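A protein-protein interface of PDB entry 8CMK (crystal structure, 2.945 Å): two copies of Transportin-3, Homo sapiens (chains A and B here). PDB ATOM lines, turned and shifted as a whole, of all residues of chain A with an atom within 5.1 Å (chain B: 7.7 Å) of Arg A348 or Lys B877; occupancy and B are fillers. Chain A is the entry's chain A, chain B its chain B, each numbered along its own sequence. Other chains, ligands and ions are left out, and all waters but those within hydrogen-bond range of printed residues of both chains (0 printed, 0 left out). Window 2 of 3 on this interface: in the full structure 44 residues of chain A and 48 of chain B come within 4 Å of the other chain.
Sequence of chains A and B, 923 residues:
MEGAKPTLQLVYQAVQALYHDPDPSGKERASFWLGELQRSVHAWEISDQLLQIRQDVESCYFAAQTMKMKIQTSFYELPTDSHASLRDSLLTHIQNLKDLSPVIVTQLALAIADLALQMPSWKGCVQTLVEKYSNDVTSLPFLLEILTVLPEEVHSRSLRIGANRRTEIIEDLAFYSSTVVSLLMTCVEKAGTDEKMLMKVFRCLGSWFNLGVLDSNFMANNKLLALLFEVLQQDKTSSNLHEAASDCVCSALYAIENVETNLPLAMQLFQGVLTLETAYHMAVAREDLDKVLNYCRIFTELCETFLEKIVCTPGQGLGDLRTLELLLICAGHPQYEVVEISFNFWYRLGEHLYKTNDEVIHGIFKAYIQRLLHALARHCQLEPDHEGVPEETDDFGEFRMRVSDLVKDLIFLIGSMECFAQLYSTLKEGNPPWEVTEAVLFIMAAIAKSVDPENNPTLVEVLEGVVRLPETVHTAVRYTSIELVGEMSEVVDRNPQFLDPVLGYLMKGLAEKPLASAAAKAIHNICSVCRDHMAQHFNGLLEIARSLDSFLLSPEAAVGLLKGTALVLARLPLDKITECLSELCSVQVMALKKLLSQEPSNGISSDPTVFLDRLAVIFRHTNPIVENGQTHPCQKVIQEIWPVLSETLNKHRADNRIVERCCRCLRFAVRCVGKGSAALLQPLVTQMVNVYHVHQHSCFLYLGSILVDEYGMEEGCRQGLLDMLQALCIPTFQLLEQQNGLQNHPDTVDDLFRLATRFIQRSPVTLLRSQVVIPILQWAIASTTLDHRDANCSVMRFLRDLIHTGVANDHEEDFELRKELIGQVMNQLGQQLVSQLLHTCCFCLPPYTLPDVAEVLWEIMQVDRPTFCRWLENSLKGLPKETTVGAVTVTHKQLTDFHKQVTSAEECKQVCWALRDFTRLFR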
ATOM      1  N   GLU A 257      20.895   6.999 -28.573  1.00  0.00           N
ATOM      2  CA  GLU A 257      20.469   5.919 -27.684  1.00  0.00           C
ATOM      3  C   GLU A 257      19.238   6.325 -26.857  1.00  0.00           C
ATOM      4  O   GLU A 257      18.339   5.512 -26.638  1.00  0.00           O
ATOM      5  CB  GLU A 257      21.626   5.487 -26.774  1.00  0.00           C
ATOM      6  CG  GLU A 257      21.430   4.131 -26.090  1.00  0.00           C
ATOM      7  CD  GLU A 257      20.670   4.113 -24.771  1.00  0.00           C
ATOM      8  OE1 GLU A 257      20.925   4.999 -23.920  1.00  0.00           O
ATOM      9  OE2 GLU A 257      19.860   3.176 -24.572  1.00  0.00           O
ATOM     10  N   GLU A 304      21.345  -2.992 -32.763  1.00  0.00           N
ATOM     11  CA  GLU A 304      21.903  -2.653 -31.461  1.00  0.00           C
ATOM     12  C   GLU A 304      21.251  -1.404 -30.860  1.00  0.00           C
ATOM     13  O   GLU A 304      20.971  -1.372 -29.660  1.00  0.00           O
ATOM     14  CB  GLU A 304      23.398  -2.390 -31.618  1.00  0.00           C
ATOM     15  CG  GLU A 304      24.194  -3.643 -31.932  1.00  0.00           C
ATOM     16  CD  GLU A 304      24.681  -4.395 -30.703  1.00  0.00           C
ATOM     17  OE1 GLU A 304      23.964  -4.381 -29.672  1.00  0.00           O
ATOM     18  OE2 GLU A 304      25.777  -4.997 -30.776  1.00  0.00           O
ATOM     19  N   THR A 305      21.019  -0.383 -31.695  1.00  0.00           N
ATOM     20  CA  THR A 305      20.473   0.896 -31.275  1.00  0.00           C
ATOM     21  C   THR A 305      18.998   0.777 -30.900  1.00  0.00           C
ATOM     22  O   THR A 305      18.547   1.458 -29.984  1.00  0.00           O
ATOM     23  CB  THR A 305      20.691   1.923 -32.385  1.00  0.00           C
ATOM     24  OG1 THR A 305      22.103   2.020 -32.544  1.00  0.00           O
ATOM     25  CG2 THR A 305      20.127   3.298 -32.099  1.00  0.00           C
ATOM     26  N   LEU A 307      17.299  -2.182 -30.007  1.00  0.00           N
ATOM     27  CA  LEU A 307      17.023  -3.476 -29.386  1.00  0.00           C
ATOM     28  C   LEU A 307      15.797  -3.415 -28.464  1.00  0.00           C
ATOM     29  O   LEU A 307      14.901  -4.262 -28.538  1.00  0.00           O
ATOM     30  CB  LEU A 307      18.277  -3.948 -28.631  1.00  0.00           C
ATOM     31  CG  LEU A 307      18.083  -5.242 -27.839  1.00  0.00           C
ATOM     32  CD1 LEU A 307      17.723  -6.394 -28.767  1.00  0.00           C
ATOM     33  CD2 LEU A 307      19.320  -5.601 -27.033  1.00  0.00           C
ATOM     34  N   PHE A 343      27.275 -11.212 -34.631  1.00  0.00           N
ATOM     35  CA  PHE A 343      27.262 -12.137 -33.499  1.00  0.00           C
ATOM     36  C   PHE A 343      26.923 -11.469 -32.162  1.00  0.00           C
ATOM     37  O   PHE A 343      26.066 -11.965 -31.433  1.00  0.00           O
ATOM     38  CB  PHE A 343      28.619 -12.834 -33.333  1.00  0.00           C
ATOM     39  CG  PHE A 343      28.889 -14.031 -34.213  1.00  0.00           C
ATOM     40  CD1 PHE A 343      28.002 -14.435 -35.201  1.00  0.00           C
ATOM     41  CD2 PHE A 343      30.058 -14.759 -34.052  1.00  0.00           C
ATOM     42  CE1 PHE A 343      28.283 -15.535 -36.000  1.00  0.00           C
ATOM     43  CE2 PHE A 343      30.344 -15.853 -34.854  1.00  0.00           C
ATOM     44  CZ  PHE A 343      29.458 -16.233 -35.831  1.00  0.00           C
ATOM     45  N   ASN A 344      27.645 -10.392 -31.813  1.00  0.00           N
ATOM     46  CA  ASN A 344      27.501  -9.782 -30.501  1.00  0.00           C
ATOM     47  C   ASN A 344      26.092  -9.227 -30.305  1.00  0.00           C
ATOM     48  O   ASN A 344      25.583  -9.276 -29.188  1.00  0.00           O
ATOM     49  CB  ASN A 344      28.573  -8.730 -30.222  1.00  0.00           C
ATOM     50  CG  ASN A 344      29.906  -9.343 -29.845  1.00  0.00           C
ATOM     51  OD1 ASN A 344      30.199 -10.477 -30.215  1.00  0.00           O
ATOM     52  ND2 ASN A 344      30.735  -8.599 -29.129  1.00  0.00           N
ATOM     53  N   PHE A 345      25.443  -8.751 -31.377  1.00  0.00           N
ATOM     54  CA  PHE A 345      24.023  -8.413 -31.321  1.00  0.00           C
ATOM     55  C   PHE A 345      23.152  -9.637 -30.985  1.00  0.00           C
ATOM     56  O   PHE A 345      22.273  -9.538 -30.123  1.00  0.00           O
ATOM     57  CB  PHE A 345      23.527  -7.742 -32.611  1.00  0.00           C
ATOM     58  CG  PHE A 345      22.025  -7.611 -32.644  1.00  0.00           C
ATOM     59  CD1 PHE A 345      21.382  -6.643 -31.886  1.00  0.00           C
ATOM     60  CD2 PHE A 345      21.252  -8.535 -33.325  1.00  0.00           C
ATOM     61  CE1 PHE A 345      19.998  -6.576 -31.852  1.00  0.00           C
ATOM     62  CE2 PHE A 345      19.869  -8.474 -33.283  1.00  0.00           C
ATOM     63  CZ  PHE A 345      19.242  -7.495 -32.548  1.00  0.00           C
ATOM     64  N   TRP A 346      23.397 -10.803 -31.607  1.00  0.00           N
ATOM     65  CA  TRP A 346      22.628 -12.003 -31.296  1.00  0.00           C
ATOM     66  C   TRP A 346      22.807 -12.463 -29.844  1.00  0.00           C
ATOM     67  O   TRP A 346      21.837 -12.851 -29.205  1.00  0.00           O
ATOM     68  CB  TRP A 346      22.978 -13.135 -32.263  1.00  0.00           C
ATOM     69  CG  TRP A 346      22.641 -12.879 -33.697  1.00  0.00           C
ATOM     70  CD1 TRP A 346      23.514 -12.908 -34.741  1.00  0.00           C
ATOM     71  CD2 TRP A 346      21.344 -12.626 -34.269  1.00  0.00           C
ATOM     72  NE1 TRP A 346      22.870 -12.648 -35.918  1.00  0.00           N
ATOM     73  CE2 TRP A 346      21.530 -12.496 -35.664  1.00  0.00           C
ATOM     74  CE3 TRP A 346      20.048 -12.519 -33.755  1.00  0.00           C
ATOM     75  CZ2 TRP A 346      20.467 -12.253 -36.540  1.00  0.00           C
ATOM     76  CZ3 TRP A 346      19.000 -12.280 -34.622  1.00  0.00           C
ATOM     77  CH2 TRP A 346      19.209 -12.135 -35.993  1.00  0.00           C
ATOM     78  N   TYR A 347      24.033 -12.430 -29.314  1.00  0.00           N
ATOM     79  CA  TYR A 347      24.259 -12.628 -27.891  1.00  0.00           C
ATOM     80  C   TYR A 347      23.424 -11.657 -27.050  1.00  0.00           C
ATOM     81  O   TYR A 347      22.762 -12.067 -26.097  1.00  0.00           O
ATOM     82  CB  TYR A 347      25.736 -12.427 -27.544  1.00  0.00           C
ATOM     83  CG  TYR A 347      26.673 -13.570 -27.851  1.00  0.00           C
ATOM     84  CD1 TYR A 347      26.693 -14.712 -27.067  1.00  0.00           C
ATOM     85  CD2 TYR A 347      27.589 -13.488 -28.890  1.00  0.00           C
ATOM     86  CE1 TYR A 347      27.575 -15.755 -27.318  1.00  0.00           C
ATOM     87  CE2 TYR A 347      28.488 -14.512 -29.145  1.00  0.00           C
ATOM     88  CZ  TYR A 347      28.479 -15.654 -28.362  1.00  0.00           C
ATOM     89  OH  TYR A 347      29.398 -16.642 -28.627  1.00  0.00           O
ATOM     90  N   ARG A 348      23.458 -10.365 -27.393  1.00  0.00           N
ATOM     91  CA  ARG A 348      22.787  -9.329 -26.629  1.00  0.00           C
ATOM     92  C   ARG A 348      21.263  -9.471 -26.683  1.00  0.00           C
ATOM     93  O   ARG A 348      20.596  -9.307 -25.666  1.00  0.00           O
ATOM     94  CB  ARG A 348      23.235  -7.969 -27.153  1.00  0.00           C
ATOM     95  CG  ARG A 348      22.852  -6.833 -26.226  1.00  0.00           C
ATOM     96  CD  ARG A 348      23.291  -5.499 -26.790  1.00  0.00           C
ATOM     97  NE  ARG A 348      22.740  -4.390 -26.027  1.00  0.00           N
ATOM     98  CZ  ARG A 348      22.198  -3.297 -26.551  1.00  0.00           C
ATOM     99  NH1 ARG A 348      21.519  -2.469 -25.776  1.00  0.00           N
ATOM    100  NH2 ARG A 348      22.281  -3.059 -27.849  1.00  0.00           N
ATOM    101  N   LEU A 349      20.702  -9.777 -27.858  1.00  0.00           N
ATOM    102  CA  LEU A 349      19.284 -10.079 -27.976  1.00  0.00           C
ATOM    103  C   LEU A 349      18.941 -11.286 -27.100  1.00  0.00           C
ATOM    104  O   LEU A 349      18.064 -11.188 -26.250  1.00  0.00           O
ATOM    105  CB  LEU A 349      18.947 -10.322 -29.449  1.00  0.00           C
ATOM    106  CG  LEU A 349      17.513 -10.768 -29.727  1.00  0.00           C
ATOM    107  CD1 LEU A 349      16.515  -9.670 -29.407  1.00  0.00           C
ATOM    108  CD2 LEU A 349      17.348 -11.211 -31.171  1.00  0.00           C
ATOM    109  N   GLY A 350      19.646 -12.411 -27.280  1.00  0.00           N
ATOM    110  CA  GLY A 350      19.391 -13.639 -26.534  1.00  0.00           C
ATOM    111  C   GLY A 350      19.435 -13.440 -25.017  1.00  0.00           C
ATOM    112  O   GLY A 350      18.589 -13.958 -24.295  1.00  0.00           O
ATOM    113  N   GLU A 351      20.402 -12.645 -24.553  1.00  0.00           N
ATOM    114  CA  GLU A 351      20.513 -12.254 -23.159  1.00  0.00           C
ATOM    115  C   GLU A 351      19.314 -11.420 -22.681  1.00  0.00           C
ATOM    116  O   GLU A 351      18.795 -11.680 -21.600  1.00  0.00           O
ATOM    117  CB  GLU A 351      21.843 -11.527 -22.966  1.00  0.00           C
ATOM    118  CG  GLU A 351      22.098 -11.105 -21.531  1.00  0.00           C
ATOM    119  CD  GLU A 351      22.241 -12.214 -20.496  1.00  0.00           C
ATOM    120  OE1 GLU A 351      22.591 -13.359 -20.877  1.00  0.00           O
ATOM    121  OE2 GLU A 351      21.996 -11.928 -19.296  1.00  0.00           O
ATOM    122  N   HIS A 352      18.846 -10.430 -23.457  1.00  0.00           N
ATOM    123  CA  HIS A 352      17.678  -9.645 -23.069  1.00  0.00           C
ATOM    124  C   HIS A 352      16.434 -10.518 -22.918  1.00  0.00           C
ATOM    125  O   HIS A 352      15.710 -10.380 -21.938  1.00  0.00           O
ATOM    126  CB  HIS A 352      17.415  -8.492 -24.043  1.00  0.00           C
ATOM    127  CG  HIS A 352      18.275  -7.317 -23.738  1.00  0.00           C
ATOM    128  ND1 HIS A 352      19.623  -7.233 -24.021  1.00  0.00           N
ATOM    129  CD2 HIS A 352      17.946  -6.168 -23.132  1.00  0.00           C
ATOM    130  CE1 HIS A 352      20.083  -6.063 -23.591  1.00  0.00           C
ATOM    131  NE2 HIS A 352      19.080  -5.397 -23.055  1.00  0.00           N
ATOM    132  N   GLN B 831      27.641 -12.551 -17.862  1.00  0.00           N
ATOM    133  CA  GLN B 831      27.188 -11.276 -18.388  1.00  0.00           C
ATOM    134  C   GLN B 831      26.480 -10.466 -17.295  1.00  0.00           C
ATOM    135  O   GLN B 831      26.775  -9.286 -17.119  1.00  0.00           O
ATOM    136  CB  GLN B 831      26.303 -11.511 -19.614  1.00  0.00           C
ATOM    137  CG  GLN B 831      25.779 -10.223 -20.241  1.00  0.00           C
ATOM    138  CD  GLN B 831      26.854  -9.392 -20.903  1.00  0.00           C
ATOM    139  OE1 GLN B 831      27.304  -9.696 -22.007  1.00  0.00           O
ATOM    140  NE2 GLN B 831      27.245  -8.290 -20.282  1.00  0.00           N
ATOM    141  N   LEU B 838      29.928  -3.233 -13.306  1.00  0.00           N
ATOM    142  CA  LEU B 838      30.129  -1.918 -13.888  1.00  0.00           C
ATOM    143  C   LEU B 838      29.111  -0.926 -13.329  1.00  0.00           C
ATOM    144  O   LEU B 838      29.484   0.183 -12.970  1.00  0.00           O
ATOM    145  CB  LEU B 838      30.009  -2.018 -15.409  1.00  0.00           C
ATOM    146  CG  LEU B 838      30.537  -0.812 -16.178  1.00  0.00           C
ATOM    147  CD1 LEU B 838      32.054  -0.715 -16.042  1.00  0.00           C
ATOM    148  CD2 LEU B 838      30.118  -0.886 -17.642  1.00  0.00           C
ATOM    149  N   ARG B 870      33.301  -9.222 -25.110  1.00  0.00           N
ATOM    150  CA  ARG B 870      31.883  -9.147 -25.434  1.00  0.00           C
ATOM    151  C   ARG B 870      31.046  -8.698 -24.237  1.00  0.00           C
ATOM    152  O   ARG B 870      30.142  -7.874 -24.370  1.00  0.00           O
ATOM    153  CB  ARG B 870      31.379 -10.515 -25.898  1.00  0.00           C
ATOM    154  CG  ARG B 870      29.867 -10.552 -26.057  1.00  0.00           C
ATOM    155  CD  ARG B 870      29.328 -11.756 -26.803  1.00  0.00           C
ATOM    156  NE  ARG B 870      30.168 -12.939 -26.681  1.00  0.00           N
ATOM    157  CZ  ARG B 870      29.989 -13.919 -25.802  1.00  0.00           C
ATOM    158  NH1 ARG B 870      30.861 -14.911 -25.746  1.00  0.00           N
ATOM    159  NH2 ARG B 870      28.973 -13.886 -24.957  1.00  0.00           N
ATOM    160  N   TRP B 871      31.314  -9.301 -23.077  1.00  0.00           N
ATOM    161  CA  TRP B 871      30.563  -9.019 -21.866  1.00  0.00           C
ATOM    162  C   TRP B 871      30.683  -7.547 -21.473  1.00  0.00           C
ATOM    163  O   TRP B 871      29.674  -6.914 -21.188  1.00  0.00           O
ATOM    164  CB  TRP B 871      31.016  -9.954 -20.738  1.00  0.00           C
ATOM    165  CG  TRP B 871      30.559 -11.377 -20.877  1.00  0.00           C
ATOM    166  CD1 TRP B 871      29.605 -11.870 -21.722  1.00  0.00           C
ATOM    167  CD2 TRP B 871      31.063 -12.520 -20.159  1.00  0.00           C
ATOM    168  NE1 TRP B 871      29.464 -13.223 -21.559  1.00  0.00           N
ATOM    169  CE2 TRP B 871      30.348 -13.653 -20.606  1.00  0.00           C
ATOM    170  CE3 TRP B 871      32.038 -12.698 -19.175  1.00  0.00           C
ATOM    171  CZ2 TRP B 871      30.571 -14.931 -20.086  1.00  0.00           C
ATOM    172  CZ3 TRP B 871      32.250 -13.958 -18.651  1.00  0.00           C
ATOM    173  CH2 TRP B 871      31.545 -15.062 -19.123  1.00  0.00           C
ATOM    174  N   LEU B 872      31.906  -7.001 -21.466  1.00  0.00           N
ATOM    175  CA  LEU B 872      32.106  -5.607 -21.096  1.00  0.00           C
ATOM    176  C   LEU B 872      31.430  -4.689 -22.119  1.00  0.00           C
ATOM    177  O   LEU B 872      30.758  -3.730 -21.741  1.00  0.00           O
ATOM    178  CB  LEU B 872      33.609  -5.342 -20.959  1.00  0.00           C
ATOM    179  CG  LEU B 872      34.001  -3.961 -20.422  1.00  0.00           C
ATOM    180  CD1 LEU B 872      33.548  -3.740 -18.981  1.00  0.00           C
ATOM    181  CD2 LEU B 872      35.507  -3.772 -20.522  1.00  0.00           C
ATOM    182  N   GLU B 873      31.542  -5.036 -23.408  1.00  0.00           N
ATOM    183  CA  GLU B 873      30.873  -4.339 -24.502  1.00  0.00           C
ATOM    184  C   GLU B 873      29.360  -4.258 -24.276  1.00  0.00           C
ATOM    185  O   GLU B 873      28.799  -3.168 -24.223  1.00  0.00           O
ATOM    186  CB  GLU B 873      31.221  -5.055 -25.810  1.00  0.00           C
ATOM    187  CG  GLU B 873      30.443  -4.574 -27.013  1.00  0.00           C
ATOM    188  CD  GLU B 873      30.808  -5.268 -28.319  1.00  0.00           C
ATOM    189  OE1 GLU B 873      32.010  -5.485 -28.569  1.00  0.00           O
ATOM    190  OE2 GLU B 873      29.881  -5.580 -29.094  1.00  0.00           O
ATOM    191  N   ASN B 874      28.700  -5.409 -24.127  1.00  0.00           N
ATOM    192  CA  ASN B 874      27.258  -5.440 -23.919  1.00  0.00           C
ATOM    193  C   ASN B 874      26.842  -4.799 -22.584  1.00  0.00           C
ATOM    194  O   ASN B 874      25.692  -4.365 -22.443  1.00  0.00           O
ATOM    195  CB  ASN B 874      26.736  -6.871 -24.074  1.00  0.00           C
ATOM    196  CG  ASN B 874      26.769  -7.364 -25.509  1.00  0.00           C
ATOM    197  OD1 ASN B 874      26.816  -6.577 -26.456  1.00  0.00           O
ATOM    198  ND2 ASN B 874      26.725  -8.674 -25.689  1.00  0.00           N
ATOM    199  N   SER B 875      27.775  -4.704 -21.618  1.00  0.00           N
ATOM    200  CA  SER B 875      27.559  -3.957 -20.381  1.00  0.00           C
ATOM    201  C   SER B 875      27.528  -2.460 -20.649  1.00  0.00           C
ATOM    202  O   SER B 875      26.653  -1.756 -20.151  1.00  0.00           O
ATOM    203  CB  SER B 875      28.611  -4.238 -19.353  1.00  0.00           C
ATOM    204  OG  SER B 875      28.680  -5.622 -19.099  1.00  0.00           O
ATOM    205  N   LEU B 876      28.495  -1.981 -21.433  1.00  0.00           N
ATOM    206  CA  LEU B 876      28.597  -0.570 -21.754  1.00  0.00           C
ATOM    207  C   LEU B 876      27.414  -0.108 -22.597  1.00  0.00           C
ATOM    208  O   LEU B 876      26.958   1.014 -22.407  1.00  0.00           O
ATOM    209  CB  LEU B 876      29.940  -0.340 -22.447  1.00  0.00           C
ATOM    210  CG  LEU B 876      31.127  -0.430 -21.490  1.00  0.00           C
ATOM    211  CD1 LEU B 876      32.423  -0.705 -22.223  1.00  0.00           C
ATOM    212  CD2 LEU B 876      31.244   0.847 -20.679  1.00  0.00           C
ATOM    213  N   LYS B 877      26.901  -0.969 -23.490  1.00  0.00           N
ATOM    214  CA  LYS B 877      25.681  -0.686 -24.239  1.00  0.00           C
ATOM    215  C   LYS B 877      24.456  -0.628 -23.327  1.00  0.00           C
ATOM    216  O   LYS B 877      23.596   0.224 -23.525  1.00  0.00           O
ATOM    217  CB  LYS B 877      25.424  -1.751 -25.302  1.00  0.00           C
ATOM    218  CG  LYS B 877      26.485  -1.856 -26.379  1.00  0.00           C
ATOM    219  CD  LYS B 877      26.227  -3.035 -27.265  1.00  0.00           C
ATOM    220  CE  LYS B 877      27.394  -3.347 -28.170  1.00  0.00           C
ATOM    221  NZ  LYS B 877      27.353  -4.763 -28.614  1.00  0.00           N
ATOM    222  N   GLY B 878      24.360  -1.539 -22.351  1.00  0.00           N
ATOM    223  CA  GLY B 878      23.221  -1.582 -21.442  1.00  0.00           C
ATOM    224  C   GLY B 878      23.200  -0.443 -20.418  1.00  0.00           C
ATOM    225  O   GLY B 878      22.156  -0.163 -19.825  1.00  0.00           O
ATOM    226  N   LEU B 879      24.360   0.200 -20.214  1.00  0.00           N
ATOM    227  CA  LEU B 879      24.539   1.317 -19.294  1.00  0.00           C
ATOM    228  C   LEU B 879      23.665   2.497 -19.730  1.00  0.00           C
ATOM    229  O   LEU B 879      23.609   2.829 -20.913  1.00  0.00           O
ATOM    230  CB  LEU B 879      26.033   1.672 -19.311  1.00  0.00           C
ATOM    231  CG  LEU B 879      26.662   2.132 -18.001  1.00  0.00           C
ATOM    232  CD1 LEU B 879      26.607   1.053 -16.925  1.00  0.00           C
ATOM    233  CD2 LEU B 879      28.108   2.531 -18.239  1.00  0.00           C
ATOM    234  N   PRO B 880      22.934   3.170 -18.807  1.00  0.00           N
ATOM    235  CA  PRO B 880      22.079   4.303 -19.175  1.00  0.00           C
ATOM    236  C   PRO B 880      22.867   5.559 -19.597  1.00  0.00           C
ATOM    237  O   PRO B 880      23.916   5.845 -19.022  1.00  0.00           O
ATOM    238  CB  PRO B 880      21.259   4.552 -17.898  1.00  0.00           C
ATOM    239  CG  PRO B 880      22.165   4.073 -16.777  1.00  0.00           C
ATOM    240  CD  PRO B 880      22.865   2.868 -17.370  1.00  0.00           C
ATOM    241  N   HIS B 892      29.517   7.681 -26.501  1.00  0.00           N
ATOM    242  CA  HIS B 892      29.844   6.361 -27.037  1.00  0.00           C
ATOM    243  C   HIS B 892      31.363   6.178 -27.202  1.00  0.00           C
ATOM    244  O   HIS B 892      31.899   5.085 -27.000  1.00  0.00           O
ATOM    245  CB  HIS B 892      29.087   6.154 -28.356  1.00  0.00           C
ATOM    246  CG  HIS B 892      29.078   4.754 -28.870  1.00  0.00           C
ATOM    247  ND1 HIS B 892      30.155   4.111 -29.444  1.00  0.00           N
ATOM    248  CD2 HIS B 892      28.063   3.888 -28.902  1.00  0.00           C
ATOM    249  CE1 HIS B 892      29.785   2.889 -29.806  1.00  0.00           C
ATOM    250  NE2 HIS B 892      28.519   2.732 -29.480  1.00  0.00           N
ATOM    251  N   LEU B 895      32.825   5.316 -23.819  1.00  0.00           N
ATOM    252  CA  LEU B 895      32.536   3.918 -23.517  1.00  0.00           C
ATOM    253  C   LEU B 895      33.550   3.006 -24.212  1.00  0.00           C
ATOM    254  O   LEU B 895      34.097   2.083 -23.604  1.00  0.00           O
ATOM    255  CB  LEU B 895      31.119   3.560 -23.983  1.00  0.00           C
ATOM    256  CG  LEU B 895      29.960   4.404 -23.445  1.00  0.00           C
ATOM    257  CD1 LEU B 895      28.640   3.898 -24.007  1.00  0.00           C
ATOM    258  CD2 LEU B 895      29.911   4.408 -21.921  1.00  0.00           C
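Of the 14 printed residues of chain A, 5 touch a printed residue of chain B. Printed residues of chain A that touch a printed residue of chain B: Glu A304, Asn A344, Tyr A347, Arg A348 and Glu A351. Hydrophobic or aromatic side chains of chain A that line the printed part of chain B: Tyr A347. Along chain A the printed residues that touch a printed residue of chain B span positions 304 to 351. Printed residues of chain B that touch a printed residue of chain A: Gln B831, Arg B870, Glu B873, Asn B874 and Lys B877. Among the printed residues, Asp or Glu carboxylates within 4 Å of a Lys or Arg side-chain nitrogen of the other chain: Glu A304 with Lys B877.
The side-chain carboxylate (OE1) of Glu A304 is in salt-bridge range of the guanidinium group (NH2) of Arg A348, 2.8 Å away. The backbone carbonyl oxygen (O) of Arg A348 lies within hydrogen-bond range of a ring nitrogen (ND1) of His A352 (2.8 Å). The backbone carbonyl oxygen (O) of Trp B871 sits at hydrogen-bond distance from the side-chain amide nitrogen (NE2) of Gln B831, at 2.9 Å. NE2 of Gln B831 sits at hydrogen-bond distance from OG of Ser B875 (3.3 Å). NZ of Lys B877 is in salt-bridge range of OE2 of Glu B873. The side-chain amide oxygen of Asn B874 is in hydrogen-bond range of the side-chain amino group of Lys B877 (2.9 Å).
NZ of Lys B877 lies within salt-bridge range of OE2 of Glu A304 (2.7 Å). ND2 of Asn A344 sits at hydrogen-bond distance from OE2 of Glu B873 (3.1 Å).
Of the printed residues of chain B, Arg A348 touches Asn B874 (3.7 Å) and Lys B877 (3.8 Å). Of the printed residues of chain A, Asn B874 touches Asn A344 (3.7 Å) and Arg A348 (3.7 Å). Printed residues of chain B within 4 Å of Asn A344: Arg B870, Glu B873 and Asn B874. Of the printed residues of chain B, Tyr A347 touches Arg B870. Of the printed residues of chain A, Arg B870 touches Asn A344 and Tyr A347.
Asn A344 touches Arg B870 (ND2 to CG, 3.7 Å). Asn A344 touches Asn B874. Tyr A347 touches Arg B870. Asn B874 touches Arg A348 (OD1 to CD, 3.7 Å). Arg A348 touches Lys B877 (CZ to CB, 3.8 Å). Glu A351 touches Gln B831.
No position is printed for both chains.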
